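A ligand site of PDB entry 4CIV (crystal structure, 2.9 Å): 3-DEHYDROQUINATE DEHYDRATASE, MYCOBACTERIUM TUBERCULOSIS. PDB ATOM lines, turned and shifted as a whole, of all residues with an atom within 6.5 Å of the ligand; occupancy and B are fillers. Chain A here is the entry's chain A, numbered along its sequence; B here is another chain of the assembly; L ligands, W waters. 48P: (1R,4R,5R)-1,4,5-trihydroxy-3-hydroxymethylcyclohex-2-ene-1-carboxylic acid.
NH1 of Arg 19 is in salt-bridge range of OAA of the ligand (3.6 Å). OAE of the ligand sits at hydrogen-bond distance from OD2 of Asp 88 of chain B (2.5 Å). The side-chain hydroxyl (OG) of Ser 103 sits at hydrogen-bond distance from an oxygen (OAA) of the ligand, at 3.1 Å. The backbone NH (N) of Ile 102 is in hydrogen-bond range of an oxygen (OAC) of the ligand, at 2.4 Å. The backbone NH (N) of Gly 78 is in hydrogen-bond range of an oxygen (OAE) of the ligand. ND1 of His 101 is in hydrogen-bond range of OAF of the ligand, 2.9 Å away. An oxygen (OAD) of the ligand lies within hydrogen-bond range of the guanidinium group (NH1) of Arg 112. NE2 of His 81 lies within hydrogen-bond range of OAD of the ligand (3.1 Å). The side-chain amide oxygen (OD1) of Asn 75 lies within hydrogen-bond range of an oxygen (OAF) of the ligand.
The side-chain amide oxygen of Asn 75 lies close to the backbone NH of Gly 77. NH2 of Arg 112 is in salt-bridge range of OD1 of Asp 88 of chain B (3.2 Å). OD1 of Asn 75 sits close to O of Val 100 (3.3 Å). O of Gly 77 is in hydrogen-bond range of OG1 of Thr 80 (2.5 Å). ND2 of Asn 75 sits at hydrogen-bond distance from OH of Tyr 133.
Gly 77 touches the ligand (C to OAE, 3.3 Å). CG1 of Val 105 touches CAI of the ligand, at 3.8 Å. Arg 108 touches the ligand. Hydrophobic or aromatic side chains that line the ligand: His 81, His 101, Ile 102 and Val 105. 12 residues have an atom within 4 Å of the ligand: Arg 19, Asn 75, Gly 77, Gly 78, His 81, His 101, Ile 102, Ser 103, Val 105, Arg 108, Arg 112 and Asp 88 of chain B. The nearest printed residue that does not touch the ligand is Pro 11 (4.1 Å).
Water W1 lies within hydrogen-bond range of OD2 of Asp 88 of chain B (2.9 Å), OAE of the ligand (3.0 Å), ND2 of Asn 12 (3.2 Å) and N of Gly 78 (3.2 Å).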
ATOM      1  N   PRO A  11     -11.684  10.725   5.697  1.00  0.00           N
ATOM      2  CA  PRO A  11     -13.018  11.193   6.061  1.00  0.00           C
ATOM      3  C   PRO A  11     -14.115  10.181   5.827  1.00  0.00           C
ATOM      4  O   PRO A  11     -14.012   9.372   4.905  1.00  0.00           O
ATOM      5  CB  PRO A  11     -13.228  12.394   5.146  1.00  0.00           C
ATOM      6  CG  PRO A  11     -11.872  12.832   4.749  1.00  0.00           C
ATOM      7  CD  PRO A  11     -11.042  11.595   4.689  1.00  0.00           C
ATOM      8  N   ASN A  12     -15.168  10.245   6.640  1.00  0.00           N
ATOM      9  CA  ASN A  12     -16.388   9.438   6.456  1.00  0.00           C
ATOM     10  C   ASN A  12     -16.188   7.931   6.608  1.00  0.00           C
ATOM     11  O   ASN A  12     -17.112   7.160   6.326  1.00  0.00           O
ATOM     12  CB  ASN A  12     -17.051   9.725   5.094  1.00  0.00           C
ATOM     13  CG  ASN A  12     -17.451  11.176   4.931  1.00  0.00           C
ATOM     14  OD1 ASN A  12     -17.857  11.828   5.877  1.00  0.00           O
ATOM     15  ND2 ASN A  12     -17.342  11.687   3.714  1.00  0.00           N
ATOM     16  N   LEU A  13     -15.000   7.504   7.039  1.00  0.00           N
ATOM     17  CA  LEU A  13     -14.730   6.086   7.259  1.00  0.00           C
ATOM     18  C   LEU A  13     -15.031   5.713   8.700  1.00  0.00           C
ATOM     19  O   LEU A  13     -14.950   4.551   9.061  1.00  0.00           O
ATOM     20  CB  LEU A  13     -13.307   5.706   6.834  1.00  0.00           C
ATOM     21  CG  LEU A  13     -13.215   5.553   5.309  1.00  0.00           C
ATOM     22  CD1 LEU A  13     -11.840   5.898   4.770  1.00  0.00           C
ATOM     23  CD2 LEU A  13     -13.666   4.171   4.836  1.00  0.00           C
ATOM     24  N   LEU A  16     -18.867   3.608   8.742  1.00  0.00           N
ATOM     25  CA  LEU A  16     -19.152   2.252   8.238  1.00  0.00           C
ATOM     26  C   LEU A  16     -20.277   1.604   9.043  1.00  0.00           C
ATOM     27  O   LEU A  16     -20.314   1.714  10.273  1.00  0.00           O
ATOM     28  CB  LEU A  16     -17.900   1.371   8.271  1.00  0.00           C
ATOM     29  CG  LEU A  16     -16.596   1.902   7.671  1.00  0.00           C
ATOM     30  CD1 LEU A  16     -15.512   0.837   7.740  1.00  0.00           C
ATOM     31  CD2 LEU A  16     -16.821   2.382   6.245  1.00  0.00           C
ATOM     32  N   ARG A  19     -23.283   4.186   7.316  1.00  0.00           N
ATOM     33  CA  ARG A  19     -23.015   4.654   5.930  1.00  0.00           C
ATOM     34  C   ARG A  19     -24.057   4.133   4.932  1.00  0.00           C
ATOM     35  O   ARG A  19     -24.431   4.827   3.975  1.00  0.00           O
ATOM     36  CB  ARG A  19     -21.600   4.220   5.477  1.00  0.00           C
ATOM     37  CG  ARG A  19     -20.786   5.265   4.730  1.00  0.00           C
ATOM     38  CD  ARG A  19     -19.312   4.854   4.625  1.00  0.00           C
ATOM     39  NE  ARG A  19     -19.110   3.602   3.866  1.00  0.00           N
ATOM     40  CZ  ARG A  19     -18.377   3.467   2.748  1.00  0.00           C
ATOM     41  NH1 ARG A  19     -17.726   4.499   2.199  1.00  0.00           N
ATOM     42  NH2 ARG A  19     -18.288   2.278   2.152  1.00  0.00           N
ATOM     43  N   ASN A  75      -6.507   4.340   3.277  1.00  0.00           N
ATOM     44  CA  ASN A  75      -7.801   4.557   2.618  1.00  0.00           C
ATOM     45  C   ASN A  75      -8.224   5.994   2.877  1.00  0.00           C
ATOM     46  O   ASN A  75      -8.931   6.260   3.846  1.00  0.00           O
ATOM     47  CB  ASN A  75      -8.851   3.589   3.161  1.00  0.00           C
ATOM     48  CG  ASN A  75     -10.217   3.755   2.494  1.00  0.00           C
ATOM     49  OD1 ASN A  75     -10.459   4.718   1.762  1.00  0.00           O
ATOM     50  ND2 ASN A  75     -11.113   2.808   2.758  1.00  0.00           N
ATOM     51  N   ALA A  76      -7.823   6.902   1.989  1.00  0.00           N
ATOM     52  CA  ALA A  76      -7.981   8.345   2.232  1.00  0.00           C
ATOM     53  C   ALA A  76      -9.381   8.908   1.950  1.00  0.00           C
ATOM     54  O   ALA A  76      -9.580  10.126   2.038  1.00  0.00           O
ATOM     55  CB  ALA A  76      -6.940   9.117   1.436  1.00  0.00           C
ATOM     56  N   GLY A  77     -10.353   8.058   1.621  1.00  0.00           N
ATOM     57  CA  GLY A  77     -11.710   8.539   1.357  1.00  0.00           C
ATOM     58  C   GLY A  77     -11.812   9.406   0.109  1.00  0.00           C
ATOM     59  O   GLY A  77     -11.159   9.148  -0.898  1.00  0.00           O
ATOM     60  N   GLY A  78     -12.638  10.454   0.183  1.00  0.00           N
ATOM     61  CA  GLY A  78     -12.832  11.380  -0.925  1.00  0.00           C
ATOM     62  C   GLY A  78     -11.646  12.310  -1.194  1.00  0.00           C
ATOM     63  O   GLY A  78     -11.628  12.995  -2.203  1.00  0.00           O
ATOM     64  N   LEU A  79     -10.681  12.331  -0.284  1.00  0.00           N
ATOM     65  CA  LEU A  79      -9.458  13.111  -0.486  1.00  0.00           C
ATOM     66  C   LEU A  79      -8.540  12.420  -1.488  1.00  0.00           C
ATOM     67  O   LEU A  79      -7.685  13.057  -2.095  1.00  0.00           O
ATOM     68  CB  LEU A  79      -8.732  13.343   0.835  1.00  0.00           C
ATOM     69  CG  LEU A  79      -9.534  14.070   1.924  1.00  0.00           C
ATOM     70  CD1 LEU A  79      -8.820  14.026   3.258  1.00  0.00           C
ATOM     71  CD2 LEU A  79      -9.836  15.507   1.519  1.00  0.00           C
ATOM     72  N   THR A  80      -8.728  11.108  -1.659  1.00  0.00           N
ATOM     73  CA  THR A  80      -8.037  10.336  -2.707  1.00  0.00           C
ATOM     74  C   THR A  80      -8.066  11.066  -4.038  1.00  0.00           C
ATOM     75  O   THR A  80      -7.044  11.233  -4.688  1.00  0.00           O
ATOM     76  CB  THR A  80      -8.746   8.975  -2.935  1.00  0.00           C
ATOM     77  OG1 THR A  80      -8.935   8.308  -1.690  1.00  0.00           O
ATOM     78  CG2 THR A  80      -7.934   8.090  -3.868  1.00  0.00           C
ATOM     79  N   HIS A  81      -9.260  11.518  -4.408  1.00  0.00           N
ATOM     80  CA  HIS A  81      -9.561  12.014  -5.751  1.00  0.00           C
ATOM     81  C   HIS A  81      -9.220  13.489  -5.943  1.00  0.00           C
ATOM     82  O   HIS A  81      -9.149  13.963  -7.085  1.00  0.00           O
ATOM     83  CB  HIS A  81     -11.046  11.808  -6.057  1.00  0.00           C
ATOM     84  CG  HIS A  81     -11.545  10.439  -5.732  1.00  0.00           C
ATOM     85  ND1 HIS A  81     -10.985   9.302  -6.270  1.00  0.00           N
ATOM     86  CD2 HIS A  81     -12.534  10.023  -4.913  1.00  0.00           C
ATOM     87  CE1 HIS A  81     -11.625   8.247  -5.812  1.00  0.00           C
ATOM     88  NE2 HIS A  81     -12.575   8.653  -4.988  1.00  0.00           N
ATOM     89  N   VAL A 100      -6.013   1.574  -0.215  1.00  0.00           N
ATOM     90  CA  VAL A 100      -7.179   0.693  -0.051  1.00  0.00           C
ATOM     91  C   VAL A 100      -8.501   1.393  -0.335  1.00  0.00           C
ATOM     92  O   VAL A 100      -8.734   2.510   0.109  1.00  0.00           O
ATOM     93  CB  VAL A 100      -7.244   0.100   1.370  1.00  0.00           C
ATOM     94  CG1 VAL A 100      -8.499  -0.764   1.531  1.00  0.00           C
ATOM     95  CG2 VAL A 100      -5.989  -0.708   1.686  1.00  0.00           C
ATOM     96  N   HIS A 101      -9.355   0.718  -1.096  1.00  0.00           N
ATOM     97  CA  HIS A 101     -10.723   1.155  -1.315  1.00  0.00           C
ATOM     98  C   HIS A 101     -11.669  -0.008  -1.054  1.00  0.00           C
ATOM     99  O   HIS A 101     -11.470  -1.094  -1.592  1.00  0.00           O
ATOM    100  CB  HIS A 101     -10.895   1.661  -2.741  1.00  0.00           C
ATOM    101  CG  HIS A 101     -10.051   2.856  -3.063  1.00  0.00           C
ATOM    102  ND1 HIS A 101     -10.410   4.131  -2.698  1.00  0.00           N
ATOM    103  CD2 HIS A 101      -8.879   2.971  -3.734  1.00  0.00           C
ATOM    104  CE1 HIS A 101      -9.490   4.988  -3.117  1.00  0.00           C
ATOM    105  NE2 HIS A 101      -8.553   4.315  -3.749  1.00  0.00           N
ATOM    106  N   ILE A 102     -12.683   0.218  -0.219  1.00  0.00           N
ATOM    107  CA  ILE A 102     -13.650  -0.810   0.157  1.00  0.00           C
ATOM    108  C   ILE A 102     -14.569  -1.083  -1.038  1.00  0.00           C
ATOM    109  O   ILE A 102     -14.650  -2.223  -1.518  1.00  0.00           O
ATOM    110  CB  ILE A 102     -14.454  -0.395   1.413  1.00  0.00           C
ATOM    111  CG1 ILE A 102     -13.571  -0.543   2.660  1.00  0.00           C
ATOM    112  CG2 ILE A 102     -15.721  -1.222   1.589  1.00  0.00           C
ATOM    113  CD1 ILE A 102     -14.174  -0.017   3.944  1.00  0.00           C
ATOM    114  N   SER A 103     -15.241  -0.049  -1.512  1.00  0.00           N
ATOM    115  CA  SER A 103     -16.084  -0.158  -2.694  1.00  0.00           C
ATOM    116  C   SER A 103     -15.191  -0.312  -3.907  1.00  0.00           C
ATOM    117  O   SER A 103     -14.012   0.060  -3.855  1.00  0.00           O
ATOM    118  CB  SER A 103     -16.948   1.103  -2.843  1.00  0.00           C
ATOM    119  OG  SER A 103     -16.148   2.273  -2.951  1.00  0.00           O
ATOM    120  N   ASN A 104     -15.721  -0.883  -4.990  1.00  0.00           N
ATOM    121  CA  ASN A 104     -15.056  -0.779  -6.280  1.00  0.00           C
ATOM    122  C   ASN A 104     -15.297   0.618  -6.824  1.00  0.00           C
ATOM    123  O   ASN A 104     -16.413   0.931  -7.220  1.00  0.00           O
ATOM    124  CB  ASN A 104     -15.560  -1.820  -7.274  1.00  0.00           C
ATOM    125  CG  ASN A 104     -14.899  -1.678  -8.644  1.00  0.00           C
ATOM    126  OD1 ASN A 104     -14.483  -0.583  -9.028  1.00  0.00           O
ATOM    127  ND2 ASN A 104     -14.807  -2.772  -9.378  1.00  0.00           N
ATOM    128  N   VAL A 105     -14.254   1.443  -6.835  1.00  0.00           N
ATOM    129  CA  VAL A 105     -14.373   2.835  -7.293  1.00  0.00           C
ATOM    130  C   VAL A 105     -14.611   2.960  -8.798  1.00  0.00           C
ATOM    131  O   VAL A 105     -15.278   3.891  -9.239  1.00  0.00           O
ATOM    132  CB  VAL A 105     -13.148   3.714  -6.890  1.00  0.00           C
ATOM    133  CG1 VAL A 105     -13.216   4.087  -5.413  1.00  0.00           C
ATOM    134  CG2 VAL A 105     -11.819   3.032  -7.219  1.00  0.00           C
ATOM    135  N   ARG A 108     -18.314   3.167 -10.327  1.00  0.00           N
ATOM    136  CA  ARG A 108     -19.135   4.235  -9.784  1.00  0.00           C
ATOM    137  C   ARG A 108     -19.032   5.465 -10.687  1.00  0.00           C
ATOM    138  O   ARG A 108     -19.082   5.321 -11.902  1.00  0.00           O
ATOM    139  CB  ARG A 108     -18.680   4.551  -8.356  1.00  0.00           C
ATOM    140  CG  ARG A 108     -18.541   3.337  -7.453  1.00  0.00           C
ATOM    141  CD  ARG A 108     -18.145   3.741  -6.048  1.00  0.00           C
ATOM    142  NE  ARG A 108     -19.124   4.680  -5.487  1.00  0.00           N
ATOM    143  CZ  ARG A 108     -18.945   5.393  -4.381  1.00  0.00           C
ATOM    144  NH1 ARG A 108     -17.840   5.308  -3.660  1.00  0.00           N
ATOM    145  NH2 ARG A 108     -19.909   6.206  -3.983  1.00  0.00           N
ATOM    146  N   PHE A 111     -15.401  10.359 -12.049  1.00  0.00           N
ATOM    147  CA  PHE A 111     -14.410  11.181 -11.341  1.00  0.00           C
ATOM    148  C   PHE A 111     -13.665  10.386 -10.273  1.00  0.00           C
ATOM    149  O   PHE A 111     -12.552  10.758  -9.880  1.00  0.00           O
ATOM    150  CB  PHE A 111     -15.050  12.447 -10.742  1.00  0.00           C
ATOM    151  CG  PHE A 111     -15.953  12.196  -9.573  1.00  0.00           C
ATOM    152  CD1 PHE A 111     -15.422  11.960  -8.319  1.00  0.00           C
ATOM    153  CD2 PHE A 111     -17.328  12.236  -9.703  1.00  0.00           C
ATOM    154  CE1 PHE A 111     -16.242  11.735  -7.234  1.00  0.00           C
ATOM    155  CE2 PHE A 111     -18.159  12.030  -8.625  1.00  0.00           C
ATOM    156  CZ  PHE A 111     -17.618  11.774  -7.381  1.00  0.00           C
ATOM    157  N   ARG A 112     -14.276   9.290  -9.807  1.00  0.00           N
ATOM    158  CA  ARG A 112     -13.659   8.383  -8.849  1.00  0.00           C
ATOM    159  C   ARG A 112     -12.531   7.540  -9.416  1.00  0.00           C
ATOM    160  O   ARG A 112     -11.813   6.888  -8.671  1.00  0.00           O
ATOM    161  CB  ARG A 112     -14.709   7.447  -8.239  1.00  0.00           C
ATOM    162  CG  ARG A 112     -15.306   7.978  -6.949  1.00  0.00           C
ATOM    163  CD  ARG A 112     -16.521   7.181  -6.507  1.00  0.00           C
ATOM    164  NE  ARG A 112     -17.582   8.081  -6.077  1.00  0.00           N
ATOM    165  CZ  ARG A 112     -17.584   8.766  -4.939  1.00  0.00           C
ATOM    166  NH1 ARG A 112     -16.585   8.657  -4.064  1.00  0.00           N
ATOM    167  NH2 ARG A 112     -18.607   9.578  -4.665  1.00  0.00           N
ATOM    168  N   TYR A 133      -7.948  -4.459   3.559  1.00  0.00           N
ATOM    169  CA  TYR A 133      -7.049  -4.106   4.666  1.00  0.00           C
ATOM    170  C   TYR A 133      -6.215  -5.312   5.102  1.00  0.00           C
ATOM    171  O   TYR A 133      -4.995  -5.204   5.225  1.00  0.00           O
ATOM    172  CB  TYR A 133      -7.826  -3.571   5.867  1.00  0.00           C
ATOM    173  CG  TYR A 133      -8.440  -2.198   5.655  1.00  0.00           C
ATOM    174  CD1 TYR A 133      -7.684  -1.048   5.861  1.00  0.00           C
ATOM    175  CD2 TYR A 133      -9.752  -2.056   5.255  1.00  0.00           C
ATOM    176  CE1 TYR A 133      -8.236   0.211   5.658  1.00  0.00           C
ATOM    177  CE2 TYR A 133     -10.315  -0.806   5.060  1.00  0.00           C
ATOM    178  CZ  TYR A 133      -9.557   0.327   5.261  1.00  0.00           C
ATOM    179  OH  TYR A 133     -10.133   1.558   5.063  1.00  0.00           O
ATOM    180  N   VAL B  84     -15.198  16.138  -2.617  1.00  0.00           N
ATOM    181  CA  VAL B  84     -15.905  14.867  -2.726  1.00  0.00           C
ATOM    182  C   VAL B  84     -16.190  14.284  -1.345  1.00  0.00           C
ATOM    183  O   VAL B  84     -17.171  13.556  -1.162  1.00  0.00           O
ATOM    184  CB  VAL B  84     -15.073  13.840  -3.518  1.00  0.00           C
ATOM    185  CG1 VAL B  84     -15.831  12.518  -3.642  1.00  0.00           C
ATOM    186  CG2 VAL B  84     -14.723  14.387  -4.882  1.00  0.00           C
ATOM    187  N   ALA B  85     -15.315  14.574  -0.382  1.00  0.00           N
ATOM    188  CA  ALA B  85     -15.529  14.168   1.000  1.00  0.00           C
ATOM    189  C   ALA B  85     -16.839  14.748   1.531  1.00  0.00           C
ATOM    190  O   ALA B  85     -17.631  14.055   2.181  1.00  0.00           O
ATOM    191  CB  ALA B  85     -14.363  14.619   1.870  1.00  0.00           C
ATOM    192  N   ASP B  88     -19.776  13.117  -0.190  1.00  0.00           N
ATOM    193  CA  ASP B  88     -20.027  11.780   0.338  1.00  0.00           C
ATOM    194  C   ASP B  88     -20.740  11.816   1.692  1.00  0.00           C
ATOM    195  O   ASP B  88     -21.485  10.905   2.019  1.00  0.00           O
ATOM    196  CB  ASP B  88     -18.724  10.981   0.452  1.00  0.00           C
ATOM    197  CG  ASP B  88     -18.434  10.153  -0.787  1.00  0.00           C
ATOM    198  OD1 ASP B  88     -19.377   9.836  -1.563  1.00  0.00           O
ATOM    199  OD2 ASP B  88     -17.249   9.791  -0.990  1.00  0.00           O
HETATM  200  OAE 48P L   1     -14.904   8.794  -0.930  1.00  0.00           O
HETATM  201  CAM 48P L   1     -15.140   7.368  -0.940  1.00  0.00           C
HETATM  202  CAL 48P L   1     -14.255   6.745  -2.040  1.00  0.00           C
HETATM  203  OAD 48P L   1     -14.724   7.150  -3.333  1.00  0.00           O
HETATM  204  CAI 48P L   1     -14.317   5.229  -1.953  1.00  0.00           C
HETATM  205  CAN 48P L   1     -13.757   4.774  -0.602  1.00  0.00           C
HETATM  206  CAJ 48P L   1     -14.152   3.451  -0.328  1.00  0.00           C
HETATM  207  OAC 48P L   1     -13.260   2.585  -0.275  1.00  0.00           O
HETATM  208  OAA 48P L   1     -15.373   3.223  -0.143  1.00  0.00           O
HETATM  209  OAF 48P L   1     -12.324   4.873  -0.635  1.00  0.00           O
HETATM  210  CAG 48P L   1     -14.193   5.573   0.458  1.00  0.00           C
HETATM  211  CAK 48P L   1     -14.855   6.799   0.323  1.00  0.00           C
HETATM  212  CAH 48P L   1     -15.213   7.441   1.505  1.00  0.00           C
HETATM  213  OAB 48P L   1     -16.218   6.624   2.117  1.00  0.00           O
HETATM  214  O   HOH W   1     -15.653  10.717   1.235  1.00  0.00           O
